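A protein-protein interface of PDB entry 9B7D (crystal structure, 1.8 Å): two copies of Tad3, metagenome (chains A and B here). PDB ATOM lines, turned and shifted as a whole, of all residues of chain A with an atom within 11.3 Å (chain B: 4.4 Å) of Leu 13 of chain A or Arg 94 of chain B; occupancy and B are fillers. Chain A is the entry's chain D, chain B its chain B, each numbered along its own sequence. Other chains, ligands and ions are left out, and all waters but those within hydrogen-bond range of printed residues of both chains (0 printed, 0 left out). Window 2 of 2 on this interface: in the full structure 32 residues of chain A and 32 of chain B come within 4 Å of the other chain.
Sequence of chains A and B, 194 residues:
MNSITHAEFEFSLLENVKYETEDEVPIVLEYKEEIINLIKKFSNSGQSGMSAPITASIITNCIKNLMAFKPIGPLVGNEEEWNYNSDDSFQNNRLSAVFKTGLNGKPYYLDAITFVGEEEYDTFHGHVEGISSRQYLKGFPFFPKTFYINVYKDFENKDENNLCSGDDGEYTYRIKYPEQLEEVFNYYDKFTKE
The backbone carbonyl oxygen of Arg 94 of chain B is in hydrogen-bond range of a ring nitrogen (NE2) of His 6 of chain A (3.0 Å).
O of Phe 69 of chain B sits at hydrogen-bond distance from NE2 of His 6 of chain A (3.3 Å).
The guanidinium group (NE) of Arg 94 of chain B lies within salt-bridge range of the side-chain carboxylate (OE2) of Glu 10 of chain A (2.9 Å).
The side-chain amide oxygen (OD1) of Asn 92 of chain B lies within hydrogen-bond range of the backbone NH (N) of Arg 94 of chain B.
NH1 of Arg 94 of chain B is in hydrogen-bond range of O of Pro 74 of chain B (3.0 Å).
The side-chain carboxylate (OE2) of Glu 81 of chain B is in salt-bridge range of the guanidinium group (NH1) of Arg 94 of chain B (3.0 Å).
O of Lys 70 of chain B touches CE1 of His 6 of chain A, at 3.0 Å.
Pro 71 of chain B touches Glu 10 of chain A.
Leu 13 of chain A touches Arg 94 of chain B (CD2 to NE, 3.3 Å).
Printed residues of chain A within 4 Å of Arg 94 of chain B: His 6, Glu 10 and Leu 13.
No residue of chain A comes within 4 Å of Asn 92 of chain B.
No residue of chain A comes within 4 Å of Asn 93 of chain B.
No residue of chain A comes within 4 Å of Leu 95 of chain B.
Printed residues of chain B within 4 Å of His 6 of chain A: Phe 69 (3.3 Å), Lys 70 (3.0 Å) and Arg 94 (3.0 Å).
Printed residues of chain B within 4 Å of Glu 10 of chain A: Pro 71 (3.4 Å) and Arg 94 (2.9 Å).
Ile 36 of chain A touches none of the printed residues of chain B.
Glu 8 of chain A touches none of the printed residues of chain B.
The nearest printed residue of chain A that does not touch Lys 70 of chain B is Glu 10 of chain A (4.6 Å).
Among the printed residues, 6 pairs touch across the chains.
Among the printed residues, Asp or Glu carboxylates within 4 Å of a Lys or Arg side-chain nitrogen of the other chain: Glu 10 of chain A with Arg 94 of chain B.
No position is printed for both chains.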
ATOM      1  N   ILE A   4       0.406 -12.749  19.866  1.00  0.00           N
ATOM      2  CA  ILE A   4       1.146 -13.048  18.648  1.00  0.00           C
ATOM      3  C   ILE A   4       0.442 -12.553  17.387  1.00  0.00           C
ATOM      4  O   ILE A   4       0.829 -12.942  16.288  1.00  0.00           O
ATOM      5  CB  ILE A   4       1.459 -14.555  18.540  1.00  0.00           C
ATOM      6  CG1 ILE A   4       0.173 -15.361  18.375  1.00  0.00           C
ATOM      7  CG2 ILE A   4       2.252 -15.012  19.748  1.00  0.00           C
ATOM      8  CD1 ILE A   4       0.387 -16.720  17.758  1.00  0.00           C
ATOM      9  N   THR A   5      -0.567 -11.681  17.518  1.00  0.00           N
ATOM     10  CA  THR A   5      -1.256 -11.148  16.338  1.00  0.00           C
ATOM     11  C   THR A   5      -0.275 -10.557  15.331  1.00  0.00           C
ATOM     12  O   THR A   5      -0.296 -10.906  14.144  1.00  0.00           O
ATOM     13  CB  THR A   5      -2.282 -10.078  16.734  1.00  0.00           C
ATOM     14  OG1 THR A   5      -3.187 -10.595  17.717  1.00  0.00           O
ATOM     15  CG2 THR A   5      -3.077  -9.639  15.506  1.00  0.00           C
ATOM     16  N   HIS A   6       0.589  -9.649  15.794  1.00  0.00           N
ATOM     17  CA  HIS A   6       1.539  -8.992  14.903  1.00  0.00           C
ATOM     18  C   HIS A   6       2.464  -9.993  14.230  1.00  0.00           C
ATOM     19  O   HIS A   6       2.644  -9.959  13.009  1.00  0.00           O
ATOM     20  CB  HIS A   6       2.365  -7.962  15.663  1.00  0.00           C
ATOM     21  CG  HIS A   6       3.308  -7.206  14.784  1.00  0.00           C
ATOM     22  ND1 HIS A   6       4.650  -7.515  14.705  1.00  0.00           N
ATOM     23  CD2 HIS A   6       3.110  -6.165  13.942  1.00  0.00           C
ATOM     24  CE1 HIS A   6       5.240  -6.696  13.853  1.00  0.00           C
ATOM     25  NE2 HIS A   6       4.329  -5.863  13.380  1.00  0.00           N
ATOM     26  N   ALA A   7       3.092 -10.868  15.019  1.00  0.00           N
ATOM     27  CA  ALA A   7       4.026 -11.839  14.450  1.00  0.00           C
ATOM     28  C   ALA A   7       3.325 -12.787  13.484  1.00  0.00           C
ATOM     29  O   ALA A   7       3.850 -13.088  12.403  1.00  0.00           O
ATOM     30  CB  ALA A   7       4.705 -12.625  15.570  1.00  0.00           C
ATOM     31  N   GLU A   8       2.145 -13.278  13.860  1.00  0.00           N
ATOM     32  CA  GLU A   8       1.423 -14.200  12.990  1.00  0.00           C
ATOM     33  C   GLU A   8       1.045 -13.530  11.676  1.00  0.00           C
ATOM     34  O   GLU A   8       1.090 -14.162  10.613  1.00  0.00           O
ATOM     35  CB  GLU A   8       0.186 -14.729  13.714  1.00  0.00           C
ATOM     36  CG  GLU A   8      -0.858 -15.369  12.820  1.00  0.00           C
ATOM     37  CD  GLU A   8      -2.200 -15.503  13.517  1.00  0.00           C
ATOM     38  OE1 GLU A   8      -2.863 -14.465  13.742  1.00  0.00           O
ATOM     39  OE2 GLU A   8      -2.589 -16.644  13.853  1.00  0.00           O
ATOM     40  N   PHE A   9       0.684 -12.247  11.720  1.00  0.00           N
ATOM     41  CA  PHE A   9       0.342 -11.562  10.478  1.00  0.00           C
ATOM     42  C   PHE A   9       1.570 -11.390   9.592  1.00  0.00           C
ATOM     43  O   PHE A   9       1.487 -11.565   8.370  1.00  0.00           O
ATOM     44  CB  PHE A   9      -0.308 -10.207  10.761  1.00  0.00           C
ATOM     45  CG  PHE A   9      -0.824  -9.527   9.520  1.00  0.00           C
ATOM     46  CD1 PHE A   9      -1.992  -9.963   8.911  1.00  0.00           C
ATOM     47  CD2 PHE A   9      -0.120  -8.489   8.936  1.00  0.00           C
ATOM     48  CE1 PHE A   9      -2.466  -9.354   7.758  1.00  0.00           C
ATOM     49  CE2 PHE A   9      -0.588  -7.872   7.784  1.00  0.00           C
ATOM     50  CZ  PHE A   9      -1.765  -8.310   7.194  1.00  0.00           C
ATOM     51  N   GLU A  10       2.722 -11.060  10.186  1.00  0.00           N
ATOM     52  CA  GLU A  10       3.930 -10.900   9.383  1.00  0.00           C
ATOM     53  C   GLU A  10       4.314 -12.203   8.689  1.00  0.00           C
ATOM     54  O   GLU A  10       4.691 -12.194   7.514  1.00  0.00           O
ATOM     55  CB  GLU A  10       5.081 -10.377  10.245  1.00  0.00           C
ATOM     56  CG  GLU A  10       4.902  -8.915  10.616  1.00  0.00           C
ATOM     57  CD  GLU A  10       4.877  -8.015   9.393  1.00  0.00           C
ATOM     58  OE1 GLU A  10       5.797  -8.114   8.550  1.00  0.00           O
ATOM     59  OE2 GLU A  10       3.906  -7.241   9.247  1.00  0.00           O
ATOM     60  N   PHE A  11       4.199 -13.336   9.385  1.00  0.00           N
ATOM     61  CA  PHE A  11       4.461 -14.607   8.714  1.00  0.00           C
ATOM     62  C   PHE A  11       3.415 -14.898   7.646  1.00  0.00           C
ATOM     63  O   PHE A  11       3.746 -15.460   6.595  1.00  0.00           O
ATOM     64  CB  PHE A  11       4.525 -15.746   9.728  1.00  0.00           C
ATOM     65  CG  PHE A  11       5.844 -15.834  10.450  1.00  0.00           C
ATOM     66  CD1 PHE A  11       6.976 -16.310   9.803  1.00  0.00           C
ATOM     67  CD2 PHE A  11       5.952 -15.425  11.769  1.00  0.00           C
ATOM     68  CE1 PHE A  11       8.191 -16.384  10.459  1.00  0.00           C
ATOM     69  CE2 PHE A  11       7.165 -15.491  12.434  1.00  0.00           C
ATOM     70  CZ  PHE A  11       8.288 -15.973  11.779  1.00  0.00           C
ATOM     71  N   SER A  12       2.158 -14.509   7.884  1.00  0.00           N
ATOM     72  CA  SER A  12       1.112 -14.759   6.896  1.00  0.00           C
ATOM     73  C   SER A  12       1.390 -14.032   5.586  1.00  0.00           C
ATOM     74  O   SER A  12       1.038 -14.536   4.513  1.00  0.00           O
ATOM     75  CB  SER A  12      -0.255 -14.356   7.455  1.00  0.00           C
ATOM     76  OG  SER A  12      -0.478 -12.964   7.315  1.00  0.00           O
ATOM     77  N   LEU A  13       2.022 -12.858   5.651  1.00  0.00           N
ATOM     78  CA  LEU A  13       2.399 -12.145   4.433  1.00  0.00           C
ATOM     79  C   LEU A  13       3.388 -12.950   3.597  1.00  0.00           C
ATOM     80  O   LEU A  13       3.329 -12.929   2.361  1.00  0.00           O
ATOM     81  CB  LEU A  13       2.992 -10.785   4.792  1.00  0.00           C
ATOM     82  CG  LEU A  13       2.081  -9.573   4.630  1.00  0.00           C
ATOM     83  CD1 LEU A  13       0.708  -9.855   5.194  1.00  0.00           C
ATOM     84  CD2 LEU A  13       2.705  -8.388   5.340  1.00  0.00           C
ATOM     85  N   LEU A  14       4.316 -13.650   4.254  1.00  0.00           N
ATOM     86  CA  LEU A  14       5.252 -14.506   3.529  1.00  0.00           C
ATOM     87  C   LEU A  14       4.563 -15.767   3.023  1.00  0.00           C
ATOM     88  O   LEU A  14       4.885 -16.269   1.939  1.00  0.00           O
ATOM     89  CB  LEU A  14       6.431 -14.872   4.436  1.00  0.00           C
ATOM     90  CG  LEU A  14       7.256 -13.721   5.015  1.00  0.00           C
ATOM     91  CD1 LEU A  14       8.491 -14.283   5.678  1.00  0.00           C
ATOM     92  CD2 LEU A  14       7.654 -12.744   3.934  1.00  0.00           C
ATOM     93  N   GLU A  15       3.617 -16.297   3.801  1.00  0.00           N
ATOM     94  CA  GLU A  15       2.958 -17.548   3.449  1.00  0.00           C
ATOM     95  C   GLU A  15       1.955 -17.373   2.313  1.00  0.00           C
ATOM     96  O   GLU A  15       1.771 -18.292   1.509  1.00  0.00           O
ATOM     97  CB  GLU A  15       2.265 -18.140   4.685  1.00  0.00           C
ATOM     98  CG  GLU A  15       3.236 -18.557   5.798  1.00  0.00           C
ATOM     99  CD  GLU A  15       2.572 -18.661   7.163  1.00  0.00           C
ATOM    100  OE1 GLU A  15       1.549 -17.976   7.394  1.00  0.00           O
ATOM    101  OE2 GLU A  15       3.083 -19.420   8.014  1.00  0.00           O
ATOM    102  N   ASN A  16       1.314 -16.210   2.220  1.00  0.00           N
ATOM    103  CA  ASN A  16       0.271 -15.974   1.222  1.00  0.00           C
ATOM    104  C   ASN A  16       0.807 -15.718  -0.187  1.00  0.00           C
ATOM    105  O   ASN A  16       0.020 -15.370  -1.073  1.00  0.00           O
ATOM    106  CB  ASN A  16      -0.618 -14.800   1.651  1.00  0.00           C
ATOM    107  CG  ASN A  16      -1.375 -15.080   2.934  1.00  0.00           C
ATOM    108  OD1 ASN A  16      -1.954 -14.177   3.542  1.00  0.00           O
ATOM    109  ND2 ASN A  16      -1.400 -16.344   3.340  1.00  0.00           N
ATOM    110  N   VAL A  17       2.100 -15.885  -0.425  1.00  0.00           N
ATOM    111  CA  VAL A  17       2.692 -15.642  -1.737  1.00  0.00           C
ATOM    112  C   VAL A  17       2.866 -16.977  -2.446  1.00  0.00           C
ATOM    113  O   VAL A  17       3.236 -17.979  -1.823  1.00  0.00           O
ATOM    114  CB  VAL A  17       4.036 -14.897  -1.603  1.00  0.00           C
ATOM    115  CG1 VAL A  17       4.755 -14.821  -2.941  1.00  0.00           C
ATOM    116  CG2 VAL A  17       3.814 -13.505  -1.036  1.00  0.00           C
ATOM    117  N   LYS A  18       2.567 -17.001  -3.746  1.00  0.00           N
ATOM    118  CA  LYS A  18       2.828 -18.178  -4.568  1.00  0.00           C
ATOM    119  C   LYS A  18       4.266 -18.125  -5.072  1.00  0.00           C
ATOM    120  O   LYS A  18       4.636 -17.202  -5.805  1.00  0.00           O
ATOM    121  CB  LYS A  18       1.860 -18.249  -5.748  1.00  0.00           C
ATOM    122  CG  LYS A  18       0.480 -18.792  -5.413  1.00  0.00           C
ATOM    123  CD  LYS A  18      -0.579 -17.707  -5.521  1.00  0.00           C
ATOM    124  CE  LYS A  18      -1.961 -18.309  -5.723  1.00  0.00           C
ATOM    125  NZ  LYS A  18      -2.867 -17.390  -6.469  1.00  0.00           N
ATOM    126  N   TYR A  19       5.074 -19.106  -4.682  1.00  0.00           N
ATOM    127  CA  TYR A  19       6.484 -19.139  -5.044  1.00  0.00           C
ATOM    128  C   TYR A  19       6.671 -20.113  -6.200  1.00  0.00           C
ATOM    129  O   TYR A  19       6.294 -21.287  -6.096  1.00  0.00           O
ATOM    130  CB  TYR A  19       7.347 -19.528  -3.843  1.00  0.00           C
ATOM    131  CG  TYR A  19       7.237 -18.527  -2.719  1.00  0.00           C
ATOM    132  CD1 TYR A  19       7.852 -17.286  -2.808  1.00  0.00           C
ATOM    133  CD2 TYR A  19       6.491 -18.810  -1.580  1.00  0.00           C
ATOM    134  CE1 TYR A  19       7.743 -16.361  -1.790  1.00  0.00           C
ATOM    135  CE2 TYR A  19       6.373 -17.888  -0.556  1.00  0.00           C
ATOM    136  CZ  TYR A  19       6.999 -16.665  -0.669  1.00  0.00           C
ATOM    137  OH  TYR A  19       6.888 -15.743   0.344  1.00  0.00           O
ATOM    138  N   GLU A  24      12.835 -19.842  -3.852  1.00  0.00           N
ATOM    139  CA  GLU A  24      12.320 -18.504  -3.586  1.00  0.00           C
ATOM    140  C   GLU A  24      11.617 -18.376  -2.238  1.00  0.00           C
ATOM    141  O   GLU A  24      11.329 -17.250  -1.813  1.00  0.00           O
ATOM    142  CB  GLU A  24      11.352 -18.084  -4.701  1.00  0.00           C
ATOM    143  CG  GLU A  24      12.012 -17.942  -6.064  1.00  0.00           C
ATOM    144  CD  GLU A  24      11.083 -17.353  -7.107  1.00  0.00           C
ATOM    145  OE1 GLU A  24      10.995 -16.109  -7.196  1.00  0.00           O
ATOM    146  OE2 GLU A  24      10.438 -18.137  -7.837  1.00  0.00           O
ATOM    147  N   VAL A  25      11.336 -19.481  -1.565  1.00  0.00           N
ATOM    148  CA  VAL A  25      10.630 -19.434  -0.277  1.00  0.00           C
ATOM    149  C   VAL A  25      11.507 -18.735   0.757  1.00  0.00           C
ATOM    150  O   VAL A  25      12.676 -19.116   0.930  1.00  0.00           O
ATOM    151  CB  VAL A  25      10.264 -20.849   0.174  1.00  0.00           C
ATOM    152  CG1 VAL A  25       9.638 -20.829   1.566  1.00  0.00           C
ATOM    153  CG2 VAL A  25       9.321 -21.506  -0.841  1.00  0.00           C
ATOM    154  N   PRO A  26      11.002 -17.719   1.460  1.00  0.00           N
ATOM    155  CA  PRO A  26      11.824 -17.030   2.466  1.00  0.00           C
ATOM    156  C   PRO A  26      12.354 -17.983   3.530  1.00  0.00           C
ATOM    157  O   PRO A  26      11.639 -18.856   4.026  1.00  0.00           O
ATOM    158  CB  PRO A  26      10.856 -16.001   3.061  1.00  0.00           C
ATOM    159  CG  PRO A  26       9.898 -15.724   1.940  1.00  0.00           C
ATOM    160  CD  PRO A  26       9.699 -17.055   1.270  1.00  0.00           C
ATOM    161  N   VAL A  28      13.129 -17.555   6.631  1.00  0.00           N
ATOM    162  CA  VAL A  28      12.602 -17.484   7.998  1.00  0.00           C
ATOM    163  C   VAL A  28      11.405 -18.395   8.219  1.00  0.00           C
ATOM    164  O   VAL A  28      11.125 -18.758   9.363  1.00  0.00           O
ATOM    165  CB  VAL A  28      12.195 -16.050   8.423  1.00  0.00           C
ATOM    166  CG1 VAL A  28      13.386 -15.254   8.892  1.00  0.00           C
ATOM    167  CG2 VAL A  28      11.415 -15.337   7.328  1.00  0.00           C
ATOM    168  N   LEU A  29      10.671 -18.759   7.159  1.00  0.00           N
ATOM    169  CA  LEU A  29       9.502 -19.620   7.345  1.00  0.00           C
ATOM    170  C   LEU A  29       9.881 -20.950   7.975  1.00  0.00           C
ATOM    171  O   LEU A  29       9.074 -21.548   8.701  1.00  0.00           O
ATOM    172  CB  LEU A  29       8.796 -19.858   6.007  1.00  0.00           C
ATOM    173  CG  LEU A  29       7.881 -18.724   5.545  1.00  0.00           C
ATOM    174  CD1 LEU A  29       7.140 -19.107   4.271  1.00  0.00           C
ATOM    175  CD2 LEU A  29       6.897 -18.329   6.646  1.00  0.00           C
ATOM    176  N   LYS A  32       9.427 -20.587  11.846  1.00  0.00           N
ATOM    177  CA  LYS A  32       8.234 -19.916  12.356  1.00  0.00           C
ATOM    178  C   LYS A  32       7.871 -20.395  13.757  1.00  0.00           C
ATOM    179  O   LYS A  32       7.654 -19.580  14.663  1.00  0.00           O
ATOM    180  CB  LYS A  32       7.062 -20.133  11.399  1.00  0.00           C
ATOM    181  CG  LYS A  32       5.746 -19.573  11.899  1.00  0.00           C
ATOM    182  CD  LYS A  32       4.671 -19.656  10.826  1.00  0.00           C
ATOM    183  CE  LYS A  32       3.356 -19.061  11.320  1.00  0.00           C
ATOM    184  NZ  LYS A  32       2.213 -19.458  10.450  1.00  0.00           N
ATOM    185  N   ILE A  36       7.972 -17.967  16.976  1.00  0.00           N
ATOM    186  CA  ILE A  36       6.703 -17.620  17.607  1.00  0.00           C
ATOM    187  C   ILE A  36       6.696 -18.034  19.075  1.00  0.00           C
ATOM    188  O   ILE A  36       6.181 -17.310  19.936  1.00  0.00           O
ATOM    189  CB  ILE A  36       5.538 -18.251  16.823  1.00  0.00           C
ATOM    190  CG1 ILE A  36       5.355 -17.524  15.491  1.00  0.00           C
ATOM    191  CG2 ILE A  36       4.247 -18.203  17.634  1.00  0.00           C
ATOM    192  CD1 ILE A  36       4.609 -16.223  15.597  1.00  0.00           C
ATOM    193  N   PHE B  69       7.707  -5.087  17.420  1.00  0.00           N
ATOM    194  CA  PHE B  69       6.473  -4.886  16.655  1.00  0.00           C
ATOM    195  C   PHE B  69       6.738  -4.143  15.350  1.00  0.00           C
ATOM    196  O   PHE B  69       5.905  -3.361  14.879  1.00  0.00           O
ATOM    197  CB  PHE B  69       5.410  -4.174  17.496  1.00  0.00           C
ATOM    198  CG  PHE B  69       5.130  -4.859  18.808  1.00  0.00           C
ATOM    199  CD1 PHE B  69       4.978  -6.236  18.857  1.00  0.00           C
ATOM    200  CD2 PHE B  69       5.031  -4.136  19.986  1.00  0.00           C
ATOM    201  CE1 PHE B  69       4.730  -6.884  20.058  1.00  0.00           C
ATOM    202  CE2 PHE B  69       4.775  -4.778  21.192  1.00  0.00           C
ATOM    203  CZ  PHE B  69       4.624  -6.151  21.224  1.00  0.00           C
ATOM    204  N   LYS B  70       7.906  -4.385  14.758  1.00  0.00           N
ATOM    205  CA  LYS B  70       8.254  -3.887  13.442  1.00  0.00           C
ATOM    206  C   LYS B  70       7.980  -4.954  12.394  1.00  0.00           C
ATOM    207  O   LYS B  70       8.005  -6.152  12.699  1.00  0.00           O
ATOM    208  CB  LYS B  70       9.733  -3.502  13.381  1.00  0.00           C
ATOM    209  CG  LYS B  70      10.037  -2.160  13.982  1.00  0.00           C
ATOM    210  CD  LYS B  70      11.508  -1.817  13.843  1.00  0.00           C
ATOM    211  CE  LYS B  70      12.101  -1.428  15.175  1.00  0.00           C
ATOM    212  NZ  LYS B  70      12.951  -0.206  15.063  1.00  0.00           N
ATOM    213  N   PRO B  71       7.706  -4.559  11.155  1.00  0.00           N
ATOM    214  CA  PRO B  71       7.505  -5.552  10.100  1.00  0.00           C
ATOM    215  C   PRO B  71       8.823  -6.226   9.751  1.00  0.00           C
ATOM    216  O   PRO B  71       9.908  -5.696   9.994  1.00  0.00           O
ATOM    217  CB  PRO B  71       6.968  -4.726   8.927  1.00  0.00           C
ATOM    218  CG  PRO B  71       7.491  -3.339   9.174  1.00  0.00           C
ATOM    219  CD  PRO B  71       7.515  -3.178  10.668  1.00  0.00           C
ATOM    220  N   GLY B  73       9.605  -7.053   6.645  1.00  0.00           N
ATOM    221  CA  GLY B  73      10.052  -6.377   5.454  1.00  0.00           C
ATOM    222  C   GLY B  73       9.580  -4.937   5.479  1.00  0.00           C
ATOM    223  O   GLY B  73       9.040  -4.463   6.484  1.00  0.00           O
ATOM    224  N   PRO B  74       9.755  -4.217   4.374  1.00  0.00           N
ATOM    225  CA  PRO B  74       9.326  -2.817   4.337  1.00  0.00           C
ATOM    226  C   PRO B  74       7.811  -2.691   4.276  1.00  0.00           C
ATOM    227  O   PRO B  74       7.094  -3.594   3.837  1.00  0.00           O
ATOM    228  CB  PRO B  74       9.975  -2.282   3.057  1.00  0.00           C
ATOM    229  CG  PRO B  74      10.053  -3.486   2.167  1.00  0.00           C
ATOM    230  CD  PRO B  74      10.317  -4.660   3.084  1.00  0.00           C
ATOM    231  N   LEU B  75       7.326  -1.542   4.739  1.00  0.00           N
ATOM    232  CA  LEU B  75       5.931  -1.192   4.509  1.00  0.00           C
ATOM    233  C   LEU B  75       5.680  -0.983   3.023  1.00  0.00           C
ATOM    234  O   LEU B  75       6.531  -0.456   2.300  1.00  0.00           O
ATOM    235  CB  LEU B  75       5.545   0.072   5.277  1.00  0.00           C
ATOM    236  CG  LEU B  75       5.659   0.036   6.795  1.00  0.00           C
ATOM    237  CD1 LEU B  75       5.124   1.336   7.367  1.00  0.00           C
ATOM    238  CD2 LEU B  75       4.875  -1.150   7.333  1.00  0.00           C
ATOM    239  N   VAL B  76       4.499  -1.402   2.574  1.00  0.00           N
ATOM    240  CA  VAL B  76       4.084  -1.266   1.184  1.00  0.00           C
ATOM    241  C   VAL B  76       3.225  -0.014   1.045  1.00  0.00           C
ATOM    242  O   VAL B  76       3.244   0.661   0.008  1.00  0.00           O
ATOM    243  CB  VAL B  76       3.328  -2.524   0.716  1.00  0.00           C
ATOM    244  CG1 VAL B  76       2.744  -2.323  -0.674  1.00  0.00           C
ATOM    245  CG2 VAL B  76       4.250  -3.730   0.743  1.00  0.00           C
ATOM    246  N   GLU B  81      -2.953  -1.989   4.311  1.00  0.00           N
ATOM    247  CA  GLU B  81      -2.012  -1.759   5.400  1.00  0.00           C
ATOM    248  C   GLU B  81      -2.484  -0.736   6.429  1.00  0.00           C
ATOM    249  O   GLU B  81      -1.748  -0.469   7.380  1.00  0.00           O
ATOM    250  CB  GLU B  81      -0.655  -1.304   4.845  1.00  0.00           C
ATOM    251  CG  GLU B  81       0.533  -2.088   5.388  1.00  0.00           C
ATOM    252  CD  GLU B  81       1.849  -1.671   4.756  1.00  0.00           C
ATOM    253  OE1 GLU B  81       2.150  -0.456   4.736  1.00  0.00           O
ATOM    254  OE2 GLU B  81       2.571  -2.560   4.254  1.00  0.00           O
ATOM    255  N   ASN B  92      -1.041   2.728  10.632  1.00  0.00           N
ATOM    256  CA  ASN B  92      -0.549   1.587   9.870  1.00  0.00           C
ATOM    257  C   ASN B  92      -0.662   0.305  10.692  1.00  0.00           C
ATOM    258  O   ASN B  92      -0.283   0.273  11.867  1.00  0.00           O
ATOM    259  CB  ASN B  92       0.901   1.817   9.446  1.00  0.00           C
ATOM    260  CG  ASN B  92       1.358   0.832   8.380  1.00  0.00           C
ATOM    261  OD1 ASN B  92       1.689  -0.317   8.681  1.00  0.00           O
ATOM    262  ND2 ASN B  92       1.354   1.274   7.123  1.00  0.00           N
ATOM    263  N   ASN B  93      -1.189  -0.755  10.064  1.00  0.00           N
ATOM    264  CA  ASN B  93      -1.431  -2.017  10.768  1.00  0.00           C
ATOM    265  C   ASN B  93      -0.138  -2.754  11.096  1.00  0.00           C
ATOM    266  O   ASN B  93      -0.095  -3.521  12.064  1.00  0.00           O
ATOM    267  CB  ASN B  93      -2.321  -2.942   9.934  1.00  0.00           C
ATOM    268  CG  ASN B  93      -3.730  -2.419   9.771  1.00  0.00           C
ATOM    269  OD1 ASN B  93      -4.280  -1.774  10.665  1.00  0.00           O
ATOM    270  ND2 ASN B  93      -4.324  -2.692   8.615  1.00  0.00           N
ATOM    271  N   ARG B  94       0.907  -2.575  10.287  1.00  0.00           N
ATOM    272  CA  ARG B  94       2.143  -3.343  10.430  1.00  0.00           C
ATOM    273  C   ARG B  94       3.234  -2.627  11.210  1.00  0.00           C
ATOM    274  O   ARG B  94       4.095  -3.287  11.804  1.00  0.00           O
ATOM    275  CB  ARG B  94       2.693  -3.701   9.048  1.00  0.00           C
ATOM    276  CG  ARG B  94       1.797  -4.594   8.213  1.00  0.00           C
ATOM    277  CD  ARG B  94       2.443  -4.749   6.862  1.00  0.00           C
ATOM    278  NE  ARG B  94       3.620  -5.602   6.917  1.00  0.00           N
ATOM    279  CZ  ARG B  94       4.582  -5.586   6.003  1.00  0.00           C
ATOM    280  NH1 ARG B  94       4.553  -4.740   4.985  1.00  0.00           N
ATOM    281  NH2 ARG B  94       5.603  -6.432   6.117  1.00  0.00           N
ATOM    282  N   LEU B  95       3.238  -1.298  11.196  1.00  0.00           N
ATOM    283  CA  LEU B  95       4.180  -0.488  11.970  1.00  0.00           C
ATOM    284  C   LEU B  95       3.335   0.616  12.597  1.00  0.00           C
ATOM    285  O   LEU B  95       3.117   1.661  11.982  1.00  0.00           O
ATOM    286  CB  LEU B  95       5.291   0.068  11.090  1.00  0.00           C
ATOM    287  CG  LEU B  95       6.386   0.864  11.807  1.00  0.00           C
ATOM    288  CD1 LEU B  95       7.157  -0.023  12.772  1.00  0.00           C
ATOM    289  CD2 LEU B  95       7.325   1.500  10.789  1.00  0.00           C
ATOM    290  N   SER B  96       2.854   0.372  13.817  1.00  0.00           N
ATOM    291  CA  SER B  96       1.755   1.178  14.341  1.00  0.00           C
ATOM    292  C   SER B  96       2.175   2.582  14.761  1.00  0.00           C
ATOM    293  O   SER B  96       1.300   3.406  15.043  1.00  0.00           O
ATOM    294  CB  SER B  96       1.083   0.444  15.507  1.00  0.00           C
ATOM    295  OG  SER B  96       1.859   0.515  16.687  1.00  0.00           O
